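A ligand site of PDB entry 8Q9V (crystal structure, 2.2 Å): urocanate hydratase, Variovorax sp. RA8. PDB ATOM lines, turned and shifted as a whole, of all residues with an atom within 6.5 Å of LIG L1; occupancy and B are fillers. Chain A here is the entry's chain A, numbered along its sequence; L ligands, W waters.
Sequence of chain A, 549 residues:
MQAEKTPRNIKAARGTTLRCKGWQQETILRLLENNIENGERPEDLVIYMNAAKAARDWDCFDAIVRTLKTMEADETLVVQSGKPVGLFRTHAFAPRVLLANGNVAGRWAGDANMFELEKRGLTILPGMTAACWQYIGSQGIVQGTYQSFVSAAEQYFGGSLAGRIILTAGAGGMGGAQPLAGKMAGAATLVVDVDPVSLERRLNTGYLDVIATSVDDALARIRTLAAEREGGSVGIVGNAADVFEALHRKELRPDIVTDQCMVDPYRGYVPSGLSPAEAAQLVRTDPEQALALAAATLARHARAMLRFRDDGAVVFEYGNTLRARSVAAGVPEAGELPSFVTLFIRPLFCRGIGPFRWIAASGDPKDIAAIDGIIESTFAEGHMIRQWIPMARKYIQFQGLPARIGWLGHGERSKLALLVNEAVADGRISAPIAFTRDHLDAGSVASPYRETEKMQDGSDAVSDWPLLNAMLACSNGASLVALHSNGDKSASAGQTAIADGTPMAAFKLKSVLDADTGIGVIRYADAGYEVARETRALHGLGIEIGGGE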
ATOM      1  N   TYR A  48      27.184 -10.351 -31.004  1.00  0.00           N
ATOM      2  CA  TYR A  48      25.785 -10.484 -31.385  1.00  0.00           C
ATOM      3  C   TYR A  48      24.966 -10.636 -30.102  1.00  0.00           C
ATOM      4  O   TYR A  48      25.513 -10.523 -28.994  1.00  0.00           O
ATOM      5  CB  TYR A  48      25.605 -11.636 -32.365  1.00  0.00           C
ATOM      6  CG  TYR A  48      25.952 -12.970 -31.776  1.00  0.00           C
ATOM      7  CD1 TYR A  48      24.991 -13.737 -31.127  1.00  0.00           C
ATOM      8  CD2 TYR A  48      27.253 -13.482 -31.899  1.00  0.00           C
ATOM      9  CE1 TYR A  48      25.303 -14.966 -30.594  1.00  0.00           C
ATOM     10  CE2 TYR A  48      27.578 -14.707 -31.362  1.00  0.00           C
ATOM     11  CZ  TYR A  48      26.602 -15.439 -30.686  1.00  0.00           C
ATOM     12  OH  TYR A  48      26.938 -16.668 -30.158  1.00  0.00           O
ATOM     13  N   MET A  49      23.645 -10.866 -30.268  1.00  0.00           N
ATOM     14  CA  MET A  49      22.605 -10.888 -29.247  1.00  0.00           C
ATOM     15  C   MET A  49      22.841  -9.823 -28.170  1.00  0.00           C
ATOM     16  O   MET A  49      22.698 -10.081 -26.957  1.00  0.00           O
ATOM     17  CB  MET A  49      22.411 -12.297 -28.624  1.00  0.00           C
ATOM     18  CG  MET A  49      23.639 -12.974 -28.033  1.00  0.00           C
ATOM     19  SD  MET A  49      23.363 -14.695 -27.434  1.00  0.00           S
ATOM     20  CE  MET A  49      22.127 -14.463 -26.183  1.00  0.00           C
ATOM     21  N   GLY A 127      27.358 -15.827 -25.160  1.00  0.00           N
ATOM     22  CA  GLY A 127      26.823 -16.392 -26.370  1.00  0.00           C
ATOM     23  C   GLY A 127      27.398 -17.801 -26.509  1.00  0.00           C
ATOM     24  O   GLY A 127      27.841 -18.431 -25.529  1.00  0.00           O
ATOM     25  N   MET A 128      27.347 -18.303 -27.727  1.00  0.00           N
ATOM     26  CA  MET A 128      28.055 -19.545 -28.057  1.00  0.00           C
ATOM     27  C   MET A 128      29.383 -19.264 -28.745  1.00  0.00           C
ATOM     28  O   MET A 128      30.422 -19.671 -28.225  1.00  0.00           O
ATOM     29  CB  MET A 128      27.146 -20.442 -28.878  1.00  0.00           C
ATOM     30  CG  MET A 128      25.992 -21.007 -28.032  1.00  0.00           C
ATOM     31  SD  MET A 128      24.960 -22.181 -28.994  1.00  0.00           S
ATOM     32  CE  MET A 128      24.343 -23.268 -27.679  1.00  0.00           C
ATOM     33  N   THR A 129      29.387 -18.531 -29.869  1.00  0.00           N
ATOM     34  CA  THR A 129      30.623 -18.307 -30.614  1.00  0.00           C
ATOM     35  C   THR A 129      31.236 -16.916 -30.382  1.00  0.00           C
ATOM     36  O   THR A 129      32.320 -16.629 -30.923  1.00  0.00           O
ATOM     37  CB  THR A 129      30.377 -18.530 -32.103  1.00  0.00           C
ATOM     38  OG1 THR A 129      29.369 -17.646 -32.558  1.00  0.00           O
ATOM     39  CG2 THR A 129      29.892 -19.960 -32.314  1.00  0.00           C
ATOM     40  N   ALA A 130      30.580 -16.061 -29.598  1.00  0.00           N
ATOM     41  CA  ALA A 130      31.091 -14.720 -29.393  1.00  0.00           C
ATOM     42  C   ALA A 130      32.366 -14.732 -28.580  1.00  0.00           C
ATOM     43  O   ALA A 130      33.393 -14.170 -29.001  1.00  0.00           O
ATOM     44  CB  ALA A 130      30.034 -13.865 -28.703  1.00  0.00           C
ATOM     45  N   ILE A 141      24.507 -18.963 -38.966  1.00  0.00           N
ATOM     46  CA  ILE A 141      23.191 -19.528 -38.708  1.00  0.00           C
ATOM     47  C   ILE A 141      22.334 -19.767 -39.984  1.00  0.00           C
ATOM     48  O   ILE A 141      21.268 -20.406 -39.898  1.00  0.00           O
ATOM     49  CB  ILE A 141      22.421 -18.608 -37.755  1.00  0.00           C
ATOM     50  CG1 ILE A 141      21.388 -19.436 -36.969  1.00  0.00           C
ATOM     51  CG2 ILE A 141      21.819 -17.431 -38.549  1.00  0.00           C
ATOM     52  CD1 ILE A 141      20.413 -18.593 -36.189  1.00  0.00           C
ATOM     53  N   MET A 174      22.182 -12.345 -35.872  1.00  0.00           N
ATOM     54  CA  MET A 174      21.720 -13.680 -36.202  1.00  0.00           C
ATOM     55  C   MET A 174      20.344 -13.679 -36.861  1.00  0.00           C
ATOM     56  O   MET A 174      20.173 -14.327 -37.901  1.00  0.00           O
ATOM     57  CB  MET A 174      21.761 -14.551 -34.954  1.00  0.00           C
ATOM     58  CG  MET A 174      23.219 -14.661 -34.430  1.00  0.00           C
ATOM     59  SD  MET A 174      24.393 -15.674 -35.376  1.00  0.00           S
ATOM     60  CE  MET A 174      24.764 -14.807 -36.942  1.00  0.00           C
ATOM     61  N   GLN A 260      12.782 -14.007 -34.214  1.00  0.00           N
ATOM     62  CA  GLN A 260      14.160 -14.136 -33.766  1.00  0.00           C
ATOM     63  C   GLN A 260      14.688 -12.812 -33.265  1.00  0.00           C
ATOM     64  O   GLN A 260      15.851 -12.476 -33.458  1.00  0.00           O
ATOM     65  CB  GLN A 260      15.047 -14.743 -34.845  1.00  0.00           C
ATOM     66  CG  GLN A 260      16.162 -15.513 -34.188  1.00  0.00           C
ATOM     67  CD  GLN A 260      17.256 -15.897 -35.152  1.00  0.00           C
ATOM     68  OE1 GLN A 260      17.028 -15.970 -36.355  1.00  0.00           O
ATOM     69  NE2 GLN A 260      18.445 -16.163 -34.624  1.00  0.00           N
ATOM     70  N   GLY A 319      14.373 -20.407 -31.321  1.00  0.00           N
ATOM     71  CA  GLY A 319      15.589 -20.478 -30.547  1.00  0.00           C
ATOM     72  C   GLY A 319      15.988 -19.234 -29.800  1.00  0.00           C
ATOM     73  O   GLY A 319      17.160 -19.084 -29.446  1.00  0.00           O
ATOM     74  N   THR A 321      14.163 -18.086 -26.962  1.00  0.00           N
ATOM     75  CA  THR A 321      13.509 -18.145 -25.638  1.00  0.00           C
ATOM     76  C   THR A 321      12.181 -17.407 -25.602  1.00  0.00           C
ATOM     77  O   THR A 321      11.696 -17.103 -24.517  1.00  0.00           O
ATOM     78  CB  THR A 321      14.377 -17.589 -24.490  1.00  0.00           C
ATOM     79  OG1 THR A 321      15.762 -17.872 -24.726  1.00  0.00           O
ATOM     80  CG2 THR A 321      13.971 -18.251 -23.103  1.00  0.00           C
ATOM     81  N   ASP A 438      28.969 -23.927 -34.521  1.00  0.00           N
ATOM     82  CA  ASP A 438      28.180 -23.373 -33.432  1.00  0.00           C
ATOM     83  C   ASP A 438      28.072 -24.433 -32.320  1.00  0.00           C
ATOM     84  O   ASP A 438      28.470 -25.585 -32.488  1.00  0.00           O
ATOM     85  CB  ASP A 438      26.811 -22.944 -33.960  1.00  0.00           C
ATOM     86  CG  ASP A 438      26.072 -21.995 -33.003  1.00  0.00           C
ATOM     87  OD1 ASP A 438      26.705 -21.402 -32.081  1.00  0.00           O
ATOM     88  OD2 ASP A 438      24.817 -21.846 -33.163  1.00  0.00           O
ATOM     89  N   HIS A 439      27.563 -24.046 -31.156  1.00  0.00           N
ATOM     90  CA  HIS A 439      27.399 -25.011 -30.074  1.00  0.00           C
ATOM     91  C   HIS A 439      26.023 -25.644 -30.112  1.00  0.00           C
ATOM     92  O   HIS A 439      25.728 -26.528 -29.305  1.00  0.00           O
ATOM     93  CB  HIS A 439      27.626 -24.371 -28.695  1.00  0.00           C
ATOM     94  CG  HIS A 439      28.957 -23.706 -28.575  1.00  0.00           C
ATOM     95  ND1 HIS A 439      29.444 -23.235 -27.369  1.00  0.00           N
ATOM     96  CD2 HIS A 439      29.909 -23.443 -29.503  1.00  0.00           C
ATOM     97  CE1 HIS A 439      30.635 -22.691 -27.566  1.00  0.00           C
ATOM     98  NE2 HIS A 439      30.947 -22.806 -28.856  1.00  0.00           N
ATOM     99  N   LEU A 440      25.187 -25.189 -31.038  1.00  0.00           N
ATOM    100  CA  LEU A 440      23.902 -25.801 -31.334  1.00  0.00           C
ATOM    101  C   LEU A 440      24.169 -27.074 -32.145  1.00  0.00           C
ATOM    102  O   LEU A 440      24.075 -27.110 -33.372  1.00  0.00           O
ATOM    103  CB  LEU A 440      23.023 -24.825 -32.095  1.00  0.00           C
ATOM    104  CG  LEU A 440      21.678 -25.442 -32.439  1.00  0.00           C
ATOM    105  CD1 LEU A 440      20.599 -24.446 -32.004  1.00  0.00           C
ATOM    106  CD2 LEU A 440      21.574 -25.814 -33.933  1.00  0.00           C
ATOM    107  N   SER A 447      20.082 -27.914 -22.978  1.00  0.00           N
ATOM    108  CA  SER A 447      19.256 -26.695 -23.062  1.00  0.00           C
ATOM    109  C   SER A 447      17.758 -27.022 -23.145  1.00  0.00           C
ATOM    110  O   SER A 447      17.222 -27.229 -24.254  1.00  0.00           O
ATOM    111  CB  SER A 447      19.651 -25.846 -24.277  1.00  0.00           C
ATOM    112  OG  SER A 447      18.991 -24.584 -24.291  1.00  0.00           O
ATOM    113  N   ARG A 450      15.402 -25.345 -25.512  1.00  0.00           N
ATOM    114  CA  ARG A 450      15.741 -25.340 -26.923  1.00  0.00           C
ATOM    115  C   ARG A 450      16.250 -26.701 -27.393  1.00  0.00           C
ATOM    116  O   ARG A 450      15.423 -27.595 -27.633  1.00  0.00           O
ATOM    117  CB  ARG A 450      16.748 -24.228 -27.231  1.00  0.00           C
ATOM    118  CG  ARG A 450      16.626 -23.762 -28.706  1.00  0.00           C
ATOM    119  CD  ARG A 450      17.550 -22.579 -29.058  1.00  0.00           C
ATOM    120  NE  ARG A 450      18.974 -22.865 -28.851  1.00  0.00           N
ATOM    121  CZ  ARG A 450      19.937 -21.996 -29.072  1.00  0.00           C
ATOM    122  NH1 ARG A 450      19.628 -20.770 -29.510  1.00  0.00           N
ATOM    123  NH2 ARG A 450      21.206 -22.339 -28.884  1.00  0.00           N
ATOM    124  N   GLU A 451      17.573 -26.881 -27.479  1.00  0.00           N
ATOM    125  CA  GLU A 451      18.103 -28.084 -28.158  1.00  0.00           C
ATOM    126  C   GLU A 451      17.602 -29.377 -27.535  1.00  0.00           C
ATOM    127  O   GLU A 451      17.427 -30.382 -28.233  1.00  0.00           O
ATOM    128  CB  GLU A 451      19.629 -28.107 -28.146  1.00  0.00           C
ATOM    129  CG  GLU A 451      20.229 -27.083 -29.121  1.00  0.00           C
ATOM    130  CD  GLU A 451      20.537 -25.764 -28.419  1.00  0.00           C
ATOM    131  OE1 GLU A 451      19.661 -25.234 -27.695  1.00  0.00           O
ATOM    132  OE2 GLU A 451      21.665 -25.281 -28.615  1.00  0.00           O
ATOM    133  N   SER A 485      28.106 -20.982 -20.456  1.00  0.00           N
ATOM    134  CA  SER A 485      26.723 -21.094 -19.982  1.00  0.00           C
ATOM    135  C   SER A 485      25.954 -19.860 -20.409  1.00  0.00           C
ATOM    136  O   SER A 485      26.512 -18.761 -20.571  1.00  0.00           O
ATOM    137  CB  SER A 485      26.584 -21.183 -18.450  1.00  0.00           C
ATOM    138  OG  SER A 485      27.137 -22.379 -17.969  1.00  0.00           O
ATOM    139  N   ASN A 486      24.654 -20.048 -20.495  1.00  0.00           N
ATOM    140  CA  ASN A 486      23.733 -18.928 -20.648  1.00  0.00           C
ATOM    141  C   ASN A 486      22.894 -18.890 -19.374  1.00  0.00           C
ATOM    142  O   ASN A 486      21.807 -19.470 -19.310  1.00  0.00           O
ATOM    143  CB  ASN A 486      22.887 -19.076 -21.919  1.00  0.00           C
ATOM    144  CG  ASN A 486      21.970 -17.864 -22.154  1.00  0.00           C
ATOM    145  OD1 ASN A 486      22.256 -16.748 -21.656  1.00  0.00           O
ATOM    146  ND2 ASN A 486      20.868 -18.071 -22.844  1.00  0.00           N
ATOM    147  N   SER A 490      21.326 -22.985 -19.817  1.00  0.00           N
ATOM    148  CA  SER A 490      21.958 -23.944 -20.707  1.00  0.00           C
ATOM    149  C   SER A 490      23.448 -23.906 -20.477  1.00  0.00           C
ATOM    150  O   SER A 490      23.980 -22.970 -19.882  1.00  0.00           O
ATOM    151  CB  SER A 490      21.641 -23.631 -22.182  1.00  0.00           C
ATOM    152  OG  SER A 490      22.123 -22.357 -22.540  1.00  0.00           O
ATOM    153  N   SER A 492      27.124 -25.201 -22.782  1.00  0.00           N
ATOM    154  CA  SER A 492      27.562 -25.658 -24.097  1.00  0.00           C
ATOM    155  C   SER A 492      29.084 -25.695 -24.164  1.00  0.00           C
ATOM    156  O   SER A 492      29.795 -25.050 -23.369  1.00  0.00           O
ATOM    157  CB  SER A 492      27.032 -24.774 -25.234  1.00  0.00           C
ATOM    158  OG  SER A 492      27.571 -23.451 -25.090  1.00  0.00           O
HETATM  159  O1  LIG L   1      21.119 -20.312 -26.158  1.00  0.00           O
HETATM  160  O2  LIG L   1      25.514 -18.809 -30.547  1.00  0.00           O
HETATM  161  N1  LIG L   1      23.581 -19.625 -31.534  1.00  0.00           N
HETATM  162  C1  LIG L   1      23.018 -17.916 -28.364  1.00  0.00           C
HETATM  163  C2  LIG L   1      23.419 -19.068 -29.282  1.00  0.00           C
HETATM  164  C3  LIG L   1      22.334 -19.900 -31.112  1.00  0.00           C
HETATM  165  C4  LIG L   1      24.309 -19.079 -30.516  1.00  0.00           C
HETATM  166  N2  LIG L   1      22.168 -19.570 -29.903  1.00  0.00           N
HETATM  167  C5  LIG L   1      22.207 -19.577 -26.521  1.00  0.00           C
HETATM  168  O3  LIG L   1      23.353 -19.852 -26.154  1.00  0.00           O
HETATM  169  C6  LIG L   1      21.914 -18.370 -27.373  1.00  0.00           C
HETATM  170  P1  LG2 L   2      20.799  -8.837 -31.908  1.00  0.00           P
HETATM  171  O1  LG2 L   2      20.842  -8.173 -30.587  1.00  0.00           O
HETATM  172  O2  LG2 L   2      21.953  -8.702 -32.832  1.00  0.00           O
HETATM  173  O3  LG2 L   2      19.465  -8.434 -32.678  1.00  0.00           O
HETATM  174  C1  LG2 L   2      18.173  -8.406 -32.041  1.00  0.00           C
HETATM  175  C2  LG2 L   2      17.266  -7.517 -32.852  1.00  0.00           C
HETATM  176  O4  LG2 L   2      15.953  -7.490 -32.274  1.00  0.00           O
HETATM  177  C3  LG2 L   2      17.713  -6.049 -32.957  1.00  0.00           C
HETATM  178  O5  LG2 L   2      17.973  -5.719 -34.315  1.00  0.00           O
HETATM  179  C4  LG2 L   2      16.550  -5.256 -32.350  1.00  0.00           C
HETATM  180  O6  LG2 L   2      16.322  -4.041 -33.015  1.00  0.00           O
HETATM  181  C5  LG2 L   2      15.392  -6.230 -32.529  1.00  0.00           C
HETATM  182  N1  LG2 L   2      14.267  -6.011 -31.636  1.00  0.00           N
HETATM  183  C6  LG2 L   2      14.309  -5.949 -30.267  1.00  0.00           C
HETATM  184  N2  LG2 L   2      13.149  -5.746 -29.714  1.00  0.00           N
HETATM  185  C7  LG2 L   2      12.271  -5.666 -30.787  1.00  0.00           C
HETATM  186  C8  LG2 L   2      10.895  -5.455 -30.854  1.00  0.00           C
HETATM  187  N3  LG2 L   2      10.121  -5.302 -29.779  1.00  0.00           N
HETATM  188  N4  LG2 L   2      10.318  -5.442 -32.074  1.00  0.00           N
HETATM  189  C9  LG2 L   2      11.105  -5.613 -33.151  1.00  0.00           C
HETATM  190  N5  LG2 L   2      12.418  -5.803 -33.199  1.00  0.00           N
HETATM  191  C10 LG2 L   2      12.953  -5.826 -31.980  1.00  0.00           C
HETATM  192  O7  LG2 L   2      20.527 -10.389 -31.678  1.00  0.00           O
HETATM  193  P2  LG2 L   2      20.803 -11.660 -32.603  1.00  0.00           P
HETATM  194  O8  LG2 L   2      20.125 -11.463 -33.907  1.00  0.00           O
HETATM  195  O9  LG2 L   2      22.259 -11.957 -32.603  1.00  0.00           O
HETATM  196  O10 LG2 L   2      20.048 -12.770 -31.760  1.00  0.00           O
HETATM  197  C11 LG2 L   2      18.617 -12.735 -31.641  1.00  0.00           C
HETATM  198  C12 LG2 L   2      18.149 -13.903 -30.819  1.00  0.00           C
HETATM  199  O11 LG2 L   2      18.374 -15.104 -31.558  1.00  0.00           O
HETATM  200  C13 LG2 L   2      18.835 -14.101 -29.461  1.00  0.00           C
HETATM  201  O12 LG2 L   2      17.918 -14.564 -28.492  1.00  0.00           O
HETATM  202  C14 LG2 L   2      19.830 -15.228 -29.748  1.00  0.00           C
HETATM  203  O13 LG2 L   2      20.149 -15.956 -28.579  1.00  0.00           O
HETATM  204  C15 LG2 L   2      19.007 -16.048 -30.741  1.00  0.00           C
HETATM  205  N6  LG2 L   2      19.798 -16.945 -31.630  1.00  0.00           N
HETATM  206  C16 LG2 L   2      19.296 -18.174 -31.943  1.00  0.00           C
HETATM  207  C17 LG2 L   2      19.852 -18.913 -32.953  1.00  0.00           C
HETATM  208  C18 LG2 L   2      19.138 -20.155 -33.435  1.00  0.00           C
HETATM  209  O14 LG2 L   2      19.783 -21.172 -33.669  1.00  0.00           O
HETATM  210  N7  LG2 L   2      17.821 -20.117 -33.563  1.00  0.00           N
HETATM  211  C19 LG2 L   2      21.127 -18.543 -33.408  1.00  0.00           C
HETATM  212  C20 LG2 L   2      21.693 -17.386 -32.950  1.00  0.00           C
HETATM  213  C21 LG2 L   2      20.926 -16.524 -32.233  1.00  0.00           C
HETATM  214  O   HOH W   1      20.006 -20.704 -23.566  1.00  0.00           O
HETATM  215  O   HOH W   2      23.566 -22.232 -24.636  1.00  0.00           O
HETATM  216  O   HOH W   3      18.502 -19.276 -26.791  1.00  0.00           O
HETATM  217  O   HOH W   4      20.868 -23.177 -25.791  1.00  0.00           O
HETATM  218  O   HOH W   5      25.513 -19.408 -24.342  1.00  0.00           O
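Residues that only touch LIG L1: Met 49 (3.4 Å) and Thr 129 (3.9 Å).
Six residues have an atom within 4 Å of LIG L1: Tyr 48, Met 49, Met 128, Thr 129, Asp 438 and Arg 450.
The nearest printed residue that does not touch LIG L1 is Asn 486 (4.01 Å).
Water W2 bridges OG of Ser 490 (2.5 Å) and O3 of LIG L1 (2.8 Å).
Water W1 lies within hydrogen-bond range of an oxygen (O1) of LIG L1 (2.8 Å), the side-chain amide nitrogen (ND2) of Asn 486 (2.9 Å) and the side-chain hydroxyl (OG) of Ser 490 (2.9 Å).
Water W5 lies within hydrogen-bond range of the backbone carbonyl oxygen (O) of Gly 127 and an oxygen (O3) of LIG L1.
Water W3 lies within hydrogen-bond range of O1 of LIG L1 (2.9 Å), O of Gly 319 (3.0 Å) and NH1 of Arg 450 (3.3 Å).
Water W4 lies within hydrogen-bond range of the side-chain hydroxyl of Ser 447, an oxygen (O1) of LIG L1, the side-chain carboxylate of Glu 451 and the guanidinium group of Arg 450.
The backbone NH of Met 128 sits close to an oxygen (O2) of LIG L1, 3.4 Å away.
The side-chain sulfur (SD) of Met 49 sits close to an oxygen (O13) of LG2 L2, at 3.6 Å.
O2 of LIG L1 lies within hydrogen-bond range of OH of Tyr 48.
An oxygen (O11) of LG2 L2 lies within hydrogen-bond range of the side-chain amide nitrogen of Gln 260, at 3.2 Å.
The backbone NH (N) of Met 49 is in hydrogen-bond range of an oxygen (O9) of LG2 L2 (2.9 Å).
The backbone NH of Met 174 is in hydrogen-bond range of an oxygen (O8) of LG2 L2 (3.0 Å).
The guanidinium group (NH2) of Arg 450 lies within salt-bridge range of an oxygen (O1) of LIG L1 (3.4 Å).
N1 of LIG L1 sits at hydrogen-bond distance from OD2 of Asp 438 (3.0 Å).
OE1 of Glu 451 is in salt-bridge range of NE of Arg 450, at 2.7 Å.
The backbone NH of Leu 440 sits at hydrogen-bond distance from the side-chain sulfur of Met 128.
OH of Tyr 48 lies within hydrogen-bond range of N of Thr 129 (3.1 Å).
O of Gly 319 lies within hydrogen-bond range of NH1 of Arg 450 (3.0 Å).
The side-chain hydroxyl (OH) of Tyr 48 lies within hydrogen-bond range of the backbone NH (N) of Met 128 (3.0 Å).
NE2 of His 439 sits close to O of Met 128, at 3.2 Å.
NH2 of Arg 450 sits close to SD of Met 128.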
